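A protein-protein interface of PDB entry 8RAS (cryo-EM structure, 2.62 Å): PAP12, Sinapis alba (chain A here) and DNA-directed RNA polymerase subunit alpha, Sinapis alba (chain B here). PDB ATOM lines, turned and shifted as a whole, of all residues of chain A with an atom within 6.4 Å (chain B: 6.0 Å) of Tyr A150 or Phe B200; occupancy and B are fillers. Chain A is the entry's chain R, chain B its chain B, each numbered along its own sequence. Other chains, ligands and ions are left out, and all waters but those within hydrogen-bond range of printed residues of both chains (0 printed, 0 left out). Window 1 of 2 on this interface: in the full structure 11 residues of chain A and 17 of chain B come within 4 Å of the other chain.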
ATOM      1  N   ARG A  73     -18.299 -23.260  -6.850  1.00  0.00           N
ATOM      2  CA  ARG A  73     -17.142 -22.375  -6.883  1.00  0.00           C
ATOM      3  C   ARG A  73     -17.547 -20.926  -6.648  1.00  0.00           C
ATOM      4  O   ARG A  73     -16.871 -20.198  -5.917  1.00  0.00           O
ATOM      5  CB  ARG A  73     -16.411 -22.522  -8.215  1.00  0.00           C
ATOM      6  CG  ARG A  73     -15.153 -21.688  -8.324  1.00  0.00           C
ATOM      7  CD  ARG A  73     -14.447 -21.945  -9.637  1.00  0.00           C
ATOM      8  NE  ARG A  73     -15.377 -21.934 -10.760  1.00  0.00           N
ATOM      9  CZ  ARG A  73     -15.680 -22.999 -11.488  1.00  0.00           C
ATOM     10  NH1 ARG A  73     -15.155 -24.186 -11.233  1.00  0.00           N
ATOM     11  NH2 ARG A  73     -16.533 -22.869 -12.499  1.00  0.00           N
ATOM     12  N   GLU A  77     -16.470 -18.407  -3.696  1.00  0.00           N
ATOM     13  CA  GLU A  77     -15.851 -17.122  -4.007  1.00  0.00           C
ATOM     14  C   GLU A  77     -16.554 -15.967  -3.303  1.00  0.00           C
ATOM     15  O   GLU A  77     -15.895 -15.062  -2.781  1.00  0.00           O
ATOM     16  CB  GLU A  77     -15.837 -16.891  -5.517  1.00  0.00           C
ATOM     17  CG  GLU A  77     -14.920 -17.824  -6.288  1.00  0.00           C
ATOM     18  CD  GLU A  77     -15.077 -17.677  -7.789  1.00  0.00           C
ATOM     19  OE1 GLU A  77     -15.791 -16.749  -8.225  1.00  0.00           O
ATOM     20  OE2 GLU A  77     -14.490 -18.489  -8.533  1.00  0.00           O
ATOM     21  N   SER A 147      -7.847 -15.534  -2.142  1.00  0.00           N
ATOM     22  CA  SER A 147      -7.371 -14.610  -3.159  1.00  0.00           C
ATOM     23  C   SER A 147      -7.612 -15.216  -4.534  1.00  0.00           C
ATOM     24  O   SER A 147      -8.012 -16.376  -4.668  1.00  0.00           O
ATOM     25  CB  SER A 147      -5.884 -14.281  -2.969  1.00  0.00           C
ATOM     26  OG  SER A 147      -5.104 -15.463  -2.911  1.00  0.00           O
ATOM     27  N   ASP A 148      -7.369 -14.411  -5.570  1.00  0.00           N
ATOM     28  CA  ASP A 148      -7.567 -14.856  -6.941  1.00  0.00           C
ATOM     29  C   ASP A 148      -6.260 -15.379  -7.514  1.00  0.00           C
ATOM     30  O   ASP A 148      -5.290 -14.614  -7.623  1.00  0.00           O
ATOM     31  CB  ASP A 148      -8.108 -13.720  -7.803  1.00  0.00           C
ATOM     32  CG  ASP A 148      -7.505 -12.373  -7.450  1.00  0.00           C
ATOM     33  OD1 ASP A 148      -6.467 -12.336  -6.758  1.00  0.00           O
ATOM     34  OD2 ASP A 148      -8.076 -11.344  -7.868  1.00  0.00           O
ATOM     35  N   PRO A 149      -6.183 -16.660  -7.885  1.00  0.00           N
ATOM     36  CA  PRO A 149      -4.955 -17.173  -8.511  1.00  0.00           C
ATOM     37  C   PRO A 149      -4.737 -16.670  -9.927  1.00  0.00           C
ATOM     38  O   PRO A 149      -3.642 -16.867 -10.471  1.00  0.00           O
ATOM     39  CB  PRO A 149      -5.160 -18.692  -8.493  1.00  0.00           C
ATOM     40  CG  PRO A 149      -6.637 -18.869  -8.471  1.00  0.00           C
ATOM     41  CD  PRO A 149      -7.195 -17.713  -7.695  1.00  0.00           C
ATOM     42  N   TYR A 150      -5.732 -16.030 -10.539  1.00  0.00           N
ATOM     43  CA  TYR A 150      -5.660 -15.614 -11.931  1.00  0.00           C
ATOM     44  C   TYR A 150      -5.336 -14.136 -12.094  1.00  0.00           C
ATOM     45  O   TYR A 150      -5.494 -13.597 -13.194  1.00  0.00           O
ATOM     46  CB  TYR A 150      -6.972 -15.945 -12.643  1.00  0.00           C
ATOM     47  CG  TYR A 150      -7.448 -17.358 -12.399  1.00  0.00           C
ATOM     48  CD1 TYR A 150      -6.738 -18.443 -12.891  1.00  0.00           C
ATOM     49  CD2 TYR A 150      -8.603 -17.607 -11.671  1.00  0.00           C
ATOM     50  CE1 TYR A 150      -7.165 -19.736 -12.669  1.00  0.00           C
ATOM     51  CE2 TYR A 150      -9.038 -18.896 -11.443  1.00  0.00           C
ATOM     52  CZ  TYR A 150      -8.315 -19.956 -11.945  1.00  0.00           C
ATOM     53  OH  TYR A 150      -8.747 -21.244 -11.720  1.00  0.00           O
ATOM     54  N   LYS A 151      -4.897 -13.467 -11.036  1.00  0.00           N
ATOM     55  CA  LYS A 151      -4.475 -12.080 -11.166  1.00  0.00           C
ATOM     56  C   LYS A 151      -3.237 -12.012 -12.053  1.00  0.00           C
ATOM     57  O   LYS A 151      -2.251 -12.709 -11.786  1.00  0.00           O
ATOM     58  CB  LYS A 151      -4.187 -11.472  -9.796  1.00  0.00           C
ATOM     59  CG  LYS A 151      -4.474  -9.982  -9.710  1.00  0.00           C
ATOM     60  CD  LYS A 151      -3.938  -9.384  -8.421  1.00  0.00           C
ATOM     61  CE  LYS A 151      -2.425  -9.474  -8.357  1.00  0.00           C
ATOM     62  NZ  LYS A 151      -1.893  -8.954  -7.067  1.00  0.00           N
ATOM     63  N   PRO A 152      -3.246 -11.197 -13.114  1.00  0.00           N
ATOM     64  CA  PRO A 152      -2.158 -11.193 -14.102  1.00  0.00           C
ATOM     65  C   PRO A 152      -0.943 -10.365 -13.689  1.00  0.00           C
ATOM     66  O   PRO A 152      -0.433  -9.550 -14.457  1.00  0.00           O
ATOM     67  CB  PRO A 152      -2.838 -10.615 -15.345  1.00  0.00           C
ATOM     68  CG  PRO A 152      -3.893  -9.721 -14.811  1.00  0.00           C
ATOM     69  CD  PRO A 152      -4.327 -10.264 -13.476  1.00  0.00           C
ATOM     70  N   GLY A 153      -0.468 -10.588 -12.468  1.00  0.00           N
ATOM     71  CA  GLY A 153       0.699  -9.899 -11.975  1.00  0.00           C
ATOM     72  C   GLY A 153       0.350  -8.725 -11.087  1.00  0.00           C
ATOM     73  O   GLY A 153      -0.819  -8.364 -10.922  1.00  0.00           O
ATOM     74  N   VAL B  18      -7.458 -25.716 -16.147  1.00  0.00           N
ATOM     75  CA  VAL B  18      -7.314 -25.384 -14.734  1.00  0.00           C
ATOM     76  C   VAL B  18      -8.068 -26.339 -13.819  1.00  0.00           C
ATOM     77  O   VAL B  18      -7.887 -26.270 -12.592  1.00  0.00           O
ATOM     78  CB  VAL B  18      -7.766 -23.935 -14.457  1.00  0.00           C
ATOM     79  CG1 VAL B  18      -6.788 -22.952 -15.075  1.00  0.00           C
ATOM     80  CG2 VAL B  18      -9.165 -23.706 -14.996  1.00  0.00           C
ATOM     81  N   ARG B  31     -12.392 -27.492 -16.900  1.00  0.00           N
ATOM     82  CA  ARG B  31     -12.405 -26.037 -16.912  1.00  0.00           C
ATOM     83  C   ARG B  31     -11.131 -25.551 -17.580  1.00  0.00           C
ATOM     84  O   ARG B  31     -10.038 -26.026 -17.256  1.00  0.00           O
ATOM     85  CB  ARG B  31     -12.522 -25.474 -15.493  1.00  0.00           C
ATOM     86  CG  ARG B  31     -13.128 -24.085 -15.424  1.00  0.00           C
ATOM     87  CD  ARG B  31     -12.924 -23.467 -14.055  1.00  0.00           C
ATOM     88  NE  ARG B  31     -13.523 -22.142 -13.963  1.00  0.00           N
ATOM     89  CZ  ARG B  31     -13.063 -21.164 -13.196  1.00  0.00           C
ATOM     90  NH1 ARG B  31     -11.994 -21.328 -12.435  1.00  0.00           N
ATOM     91  NH2 ARG B  31     -13.693 -19.993 -13.190  1.00  0.00           N
ATOM     92  N   PHE B  32     -11.269 -24.612 -18.512  1.00  0.00           N
ATOM     93  CA  PHE B  32     -10.155 -24.157 -19.326  1.00  0.00           C
ATOM     94  C   PHE B  32     -10.064 -22.641 -19.280  1.00  0.00           C
ATOM     95  O   PHE B  32     -11.045 -21.943 -19.021  1.00  0.00           O
ATOM     96  CB  PHE B  32     -10.287 -24.638 -20.776  1.00  0.00           C
ATOM     97  CG  PHE B  32     -10.518 -26.111 -20.900  1.00  0.00           C
ATOM     98  CD1 PHE B  32      -9.451 -26.983 -21.004  1.00  0.00           C
ATOM     99  CD2 PHE B  32     -11.800 -26.627 -20.903  1.00  0.00           C
ATOM    100  CE1 PHE B  32      -9.659 -28.337 -21.112  1.00  0.00           C
ATOM    101  CE2 PHE B  32     -12.011 -27.979 -21.010  1.00  0.00           C
ATOM    102  CZ  PHE B  32     -10.939 -28.835 -21.115  1.00  0.00           C
ATOM    103  N   ILE B  33      -8.861 -22.142 -19.543  1.00  0.00           N
ATOM    104  CA  ILE B  33      -8.551 -20.726 -19.430  1.00  0.00           C
ATOM    105  C   ILE B  33      -7.946 -20.250 -20.742  1.00  0.00           C
ATOM    106  O   ILE B  33      -7.404 -21.040 -21.521  1.00  0.00           O
ATOM    107  CB  ILE B  33      -7.594 -20.459 -18.245  1.00  0.00           C
ATOM    108  CG1 ILE B  33      -7.781 -19.046 -17.703  1.00  0.00           C
ATOM    109  CG2 ILE B  33      -6.147 -20.682 -18.650  1.00  0.00           C
ATOM    110  CD1 ILE B  33      -6.804 -18.689 -16.609  1.00  0.00           C
ATOM    111  N   LEU B  34      -8.066 -18.950 -21.000  1.00  0.00           N
ATOM    112  CA  LEU B  34      -7.475 -18.341 -22.186  1.00  0.00           C
ATOM    113  C   LEU B  34      -7.224 -16.872 -21.892  1.00  0.00           C
ATOM    114  O   LEU B  34      -8.173 -16.110 -21.694  1.00  0.00           O
ATOM    115  CB  LEU B  34      -8.382 -18.503 -23.408  1.00  0.00           C
ATOM    116  CG  LEU B  34      -7.853 -17.935 -24.727  1.00  0.00           C
ATOM    117  CD1 LEU B  34      -6.777 -18.830 -25.313  1.00  0.00           C
ATOM    118  CD2 LEU B  34      -8.983 -17.739 -25.722  1.00  0.00           C
ATOM    119  N   ASN B 183     -20.363 -23.625 -20.588  1.00  0.00           N
ATOM    120  CA  ASN B 183     -20.517 -22.286 -20.046  1.00  0.00           C
ATOM    121  C   ASN B 183     -19.230 -21.506 -20.263  1.00  0.00           C
ATOM    122  O   ASN B 183     -18.151 -22.082 -20.414  1.00  0.00           O
ATOM    123  CB  ASN B 183     -20.859 -22.317 -18.552  1.00  0.00           C
ATOM    124  CG  ASN B 183     -22.344 -22.208 -18.292  1.00  0.00           C
ATOM    125  OD1 ASN B 183     -22.993 -21.257 -18.725  1.00  0.00           O
ATOM    126  ND2 ASN B 183     -22.892 -23.184 -17.579  1.00  0.00           N
ATOM    127  N   HIS B 184     -19.353 -20.182 -20.278  1.00  0.00           N
ATOM    128  CA  HIS B 184     -18.194 -19.308 -20.362  1.00  0.00           C
ATOM    129  C   HIS B 184     -18.385 -18.121 -19.428  1.00  0.00           C
ATOM    130  O   HIS B 184     -19.506 -17.665 -19.198  1.00  0.00           O
ATOM    131  CB  HIS B 184     -17.938 -18.833 -21.801  1.00  0.00           C
ATOM    132  CG  HIS B 184     -18.802 -17.689 -22.231  1.00  0.00           C
ATOM    133  ND1 HIS B 184     -18.346 -16.390 -22.281  1.00  0.00           N
ATOM    134  CD2 HIS B 184     -20.088 -17.652 -22.650  1.00  0.00           C
ATOM    135  CE1 HIS B 184     -19.316 -15.600 -22.703  1.00  0.00           C
ATOM    136  NE2 HIS B 184     -20.385 -16.342 -22.934  1.00  0.00           N
ATOM    137  N   SER B 185     -17.272 -17.634 -18.886  1.00  0.00           N
ATOM    138  CA  SER B 185     -17.279 -16.497 -17.980  1.00  0.00           C
ATOM    139  C   SER B 185     -16.055 -15.637 -18.254  1.00  0.00           C
ATOM    140  O   SER B 185     -15.052 -16.104 -18.796  1.00  0.00           O
ATOM    141  CB  SER B 185     -17.309 -16.939 -16.511  1.00  0.00           C
ATOM    142  OG  SER B 185     -16.225 -17.799 -16.210  1.00  0.00           O
ATOM    143  N   ILE B 186     -16.150 -14.367 -17.871  1.00  0.00           N
ATOM    144  CA  ILE B 186     -15.145 -13.362 -18.191  1.00  0.00           C
ATOM    145  C   ILE B 186     -14.658 -12.726 -16.896  1.00  0.00           C
ATOM    146  O   ILE B 186     -15.466 -12.322 -16.054  1.00  0.00           O
ATOM    147  CB  ILE B 186     -15.703 -12.291 -19.149  1.00  0.00           C
ATOM    148  CG1 ILE B 186     -15.609 -12.760 -20.602  1.00  0.00           C
ATOM    149  CG2 ILE B 186     -14.964 -10.973 -18.989  1.00  0.00           C
ATOM    150  CD1 ILE B 186     -16.701 -13.713 -21.024  1.00  0.00           C
ATOM    151  N   HIS B 187     -13.339 -12.648 -16.738  1.00  0.00           N
ATOM    152  CA  HIS B 187     -12.707 -11.908 -15.655  1.00  0.00           C
ATOM    153  C   HIS B 187     -11.896 -10.772 -16.258  1.00  0.00           C
ATOM    154  O   HIS B 187     -11.074 -11.003 -17.148  1.00  0.00           O
ATOM    155  CB  HIS B 187     -11.800 -12.809 -14.815  1.00  0.00           C
ATOM    156  CG  HIS B 187     -12.542 -13.758 -13.926  1.00  0.00           C
ATOM    157  ND1 HIS B 187     -13.604 -14.517 -14.367  1.00  0.00           N
ATOM    158  CD2 HIS B 187     -12.366 -14.079 -12.623  1.00  0.00           C
ATOM    159  CE1 HIS B 187     -14.055 -15.259 -13.372  1.00  0.00           C
ATOM    160  NE2 HIS B 187     -13.321 -15.013 -12.302  1.00  0.00           N
ATOM    161  N   TYR B 189      -9.361  -7.309 -15.756  1.00  0.00           N
ATOM    162  CA  TYR B 189      -8.350  -6.694 -14.910  1.00  0.00           C
ATOM    163  C   TYR B 189      -7.813  -5.452 -15.606  1.00  0.00           C
ATOM    164  O   TYR B 189      -7.910  -5.310 -16.826  1.00  0.00           O
ATOM    165  CB  TYR B 189      -7.201  -7.662 -14.602  1.00  0.00           C
ATOM    166  CG  TYR B 189      -7.620  -8.898 -13.846  1.00  0.00           C
ATOM    167  CD1 TYR B 189      -8.044 -10.034 -14.517  1.00  0.00           C
ATOM    168  CD2 TYR B 189      -7.589  -8.932 -12.460  1.00  0.00           C
ATOM    169  CE1 TYR B 189      -8.428 -11.166 -13.831  1.00  0.00           C
ATOM    170  CE2 TYR B 189      -7.971 -10.059 -11.765  1.00  0.00           C
ATOM    171  CZ  TYR B 189      -8.389 -11.173 -12.456  1.00  0.00           C
ATOM    172  OH  TYR B 189      -8.771 -12.303 -11.770  1.00  0.00           O
ATOM    173  N   ILE B 198      -9.825 -12.284 -19.114  1.00  0.00           N
ATOM    174  CA  ILE B 198      -9.545 -13.713 -19.115  1.00  0.00           C
ATOM    175  C   ILE B 198     -10.837 -14.459 -19.412  1.00  0.00           C
ATOM    176  O   ILE B 198     -11.899 -14.115 -18.883  1.00  0.00           O
ATOM    177  CB  ILE B 198      -8.949 -14.173 -17.768  1.00  0.00           C
ATOM    178  CG1 ILE B 198      -7.750 -13.306 -17.384  1.00  0.00           C
ATOM    179  CG2 ILE B 198      -8.542 -15.625 -17.835  1.00  0.00           C
ATOM    180  CD1 ILE B 198      -7.140 -13.671 -16.053  1.00  0.00           C
ATOM    181  N   LEU B 199     -10.744 -15.479 -20.260  1.00  0.00           N
ATOM    182  CA  LEU B 199     -11.888 -16.295 -20.642  1.00  0.00           C
ATOM    183  C   LEU B 199     -11.812 -17.646 -19.946  1.00  0.00           C
ATOM    184  O   LEU B 199     -10.766 -18.302 -19.965  1.00  0.00           O
ATOM    185  CB  LEU B 199     -11.941 -16.486 -22.159  1.00  0.00           C
ATOM    186  CG  LEU B 199     -12.984 -17.476 -22.680  1.00  0.00           C
ATOM    187  CD1 LEU B 199     -14.389 -16.977 -22.403  1.00  0.00           C
ATOM    188  CD2 LEU B 199     -12.783 -17.729 -24.157  1.00  0.00           C
ATOM    189  N   PHE B 200     -12.919 -18.053 -19.332  1.00  0.00           N
ATOM    190  CA  PHE B 200     -13.056 -19.359 -18.704  1.00  0.00           C
ATOM    191  C   PHE B 200     -14.132 -20.138 -19.442  1.00  0.00           C
ATOM    192  O   PHE B 200     -15.205 -19.598 -19.720  1.00  0.00           O
ATOM    193  CB  PHE B 200     -13.429 -19.231 -17.226  1.00  0.00           C
ATOM    194  CG  PHE B 200     -12.328 -18.690 -16.364  1.00  0.00           C
ATOM    195  CD1 PHE B 200     -11.327 -19.520 -15.898  1.00  0.00           C
ATOM    196  CD2 PHE B 200     -12.298 -17.351 -16.018  1.00  0.00           C
ATOM    197  CE1 PHE B 200     -10.317 -19.027 -15.104  1.00  0.00           C
ATOM    198  CE2 PHE B 200     -11.289 -16.852 -15.225  1.00  0.00           C
ATOM    199  CZ  PHE B 200     -10.298 -17.691 -14.768  1.00  0.00           C
ATOM    200  N   ILE B 201     -13.850 -21.397 -19.762  1.00  0.00           N
ATOM    201  CA  ILE B 201     -14.799 -22.259 -20.456  1.00  0.00           C
ATOM    202  C   ILE B 201     -14.966 -23.543 -19.660  1.00  0.00           C
ATOM    203  O   ILE B 201     -13.979 -24.209 -19.331  1.00  0.00           O
ATOM    204  CB  ILE B 201     -14.348 -22.568 -21.897  1.00  0.00           C
ATOM    205  CG1 ILE B 201     -14.342 -21.291 -22.737  1.00  0.00           C
ATOM    206  CG2 ILE B 201     -15.256 -23.610 -22.528  1.00  0.00           C
ATOM    207  CD1 ILE B 201     -13.816 -21.480 -24.137  1.00  0.00           C
ATOM    208  N   GLU B 202     -16.213 -23.887 -19.352  1.00  0.00           N
ATOM    209  CA  GLU B 202     -16.557 -25.122 -18.663  1.00  0.00           C
ATOM    210  C   GLU B 202     -17.241 -26.060 -19.643  1.00  0.00           C
ATOM    211  O   GLU B 202     -18.138 -25.643 -20.379  1.00  0.00           O
ATOM    212  CB  GLU B 202     -17.479 -24.851 -17.477  1.00  0.00           C
ATOM    213  CG  GLU B 202     -16.773 -24.436 -16.214  1.00  0.00           C
ATOM    214  CD  GLU B 202     -17.745 -24.048 -15.126  1.00  0.00           C
ATOM    215  OE1 GLU B 202     -18.791 -23.452 -15.454  1.00  0.00           O
ATOM    216  OE2 GLU B 202     -17.470 -24.347 -13.947  1.00  0.00           O
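NE of Arg B31 sits close to NH2 of Arg A73. OE2 of Glu B202 lies within salt-bridge range of NH1 of Arg A73, 3.6 Å away. The guanidinium group (NH1) of Arg B31 lies within hydrogen-bond range of the side-chain hydroxyl (OH) of Tyr A150, 3.3 Å away.
The backbone NH (N) of Phe B200 is in hydrogen-bond range of the backbone carbonyl oxygen (O) of Ser B185 (2.9 Å). The backbone carbonyl oxygen of His B187 is in hydrogen-bond range of the backbone NH of Ile B198, at 2.7 Å. O of Asn B183 sits at hydrogen-bond distance from N of Glu B202 (2.9 Å). The backbone NH (N) of Val B18 lies within hydrogen-bond range of the backbone carbonyl oxygen (O) of Arg B31 (2.8 Å).
Val B18 touches Tyr A150 (CB to OH, 3.96 Å). CD1 of Tyr A150 touches CD1 of Ile B33, at 3.7 Å. Tyr A150 touches Tyr B189. Tyr A150 touches Ile B198. Tyr A150 touches Phe B200. Pro A152 touches Tyr B189 (CD to CG, 3.6 Å).
Pro A149 touches none of the printed residues of chain B. Tyr A150 touches just these residues of chain B: Val B18, Arg B31, Ile B33, Tyr B189, Ile B198 and Phe B200. Of the printed residues of chain B, Pro A152 touches Tyr B189. Of the printed residues of chain A, Ile B198 touches Tyr A150 (3.3 Å).
Of the 16 printed residues of chain B, 7 touch a printed residue of chain A. Printed residues of chain B that touch a printed residue of chain A: Val B18, Arg B31, Ile B33, Tyr B189, Ile B198, Phe B200 and Glu B202. Hydrophobic or aromatic side chains of chain B within 4 Å of the printed part of chain A: Val B18, Ile B33, Tyr B189, Ile B198 and Phe B200. Hydrophobic or aromatic side chains of chain A within 4 Å of the printed part of chain B: Tyr A150 and Pro A152. Along chain A the printed residues that touch a printed residue of chain B span positions 73 to 152. Among the printed residues, 9 pairs touch across the chains. Among the printed residues, Asp or Glu carboxylates within 4 Å of a Lys or Arg side-chain nitrogen of the other chain: Arg A73 with Glu B202 (2.3 Å).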
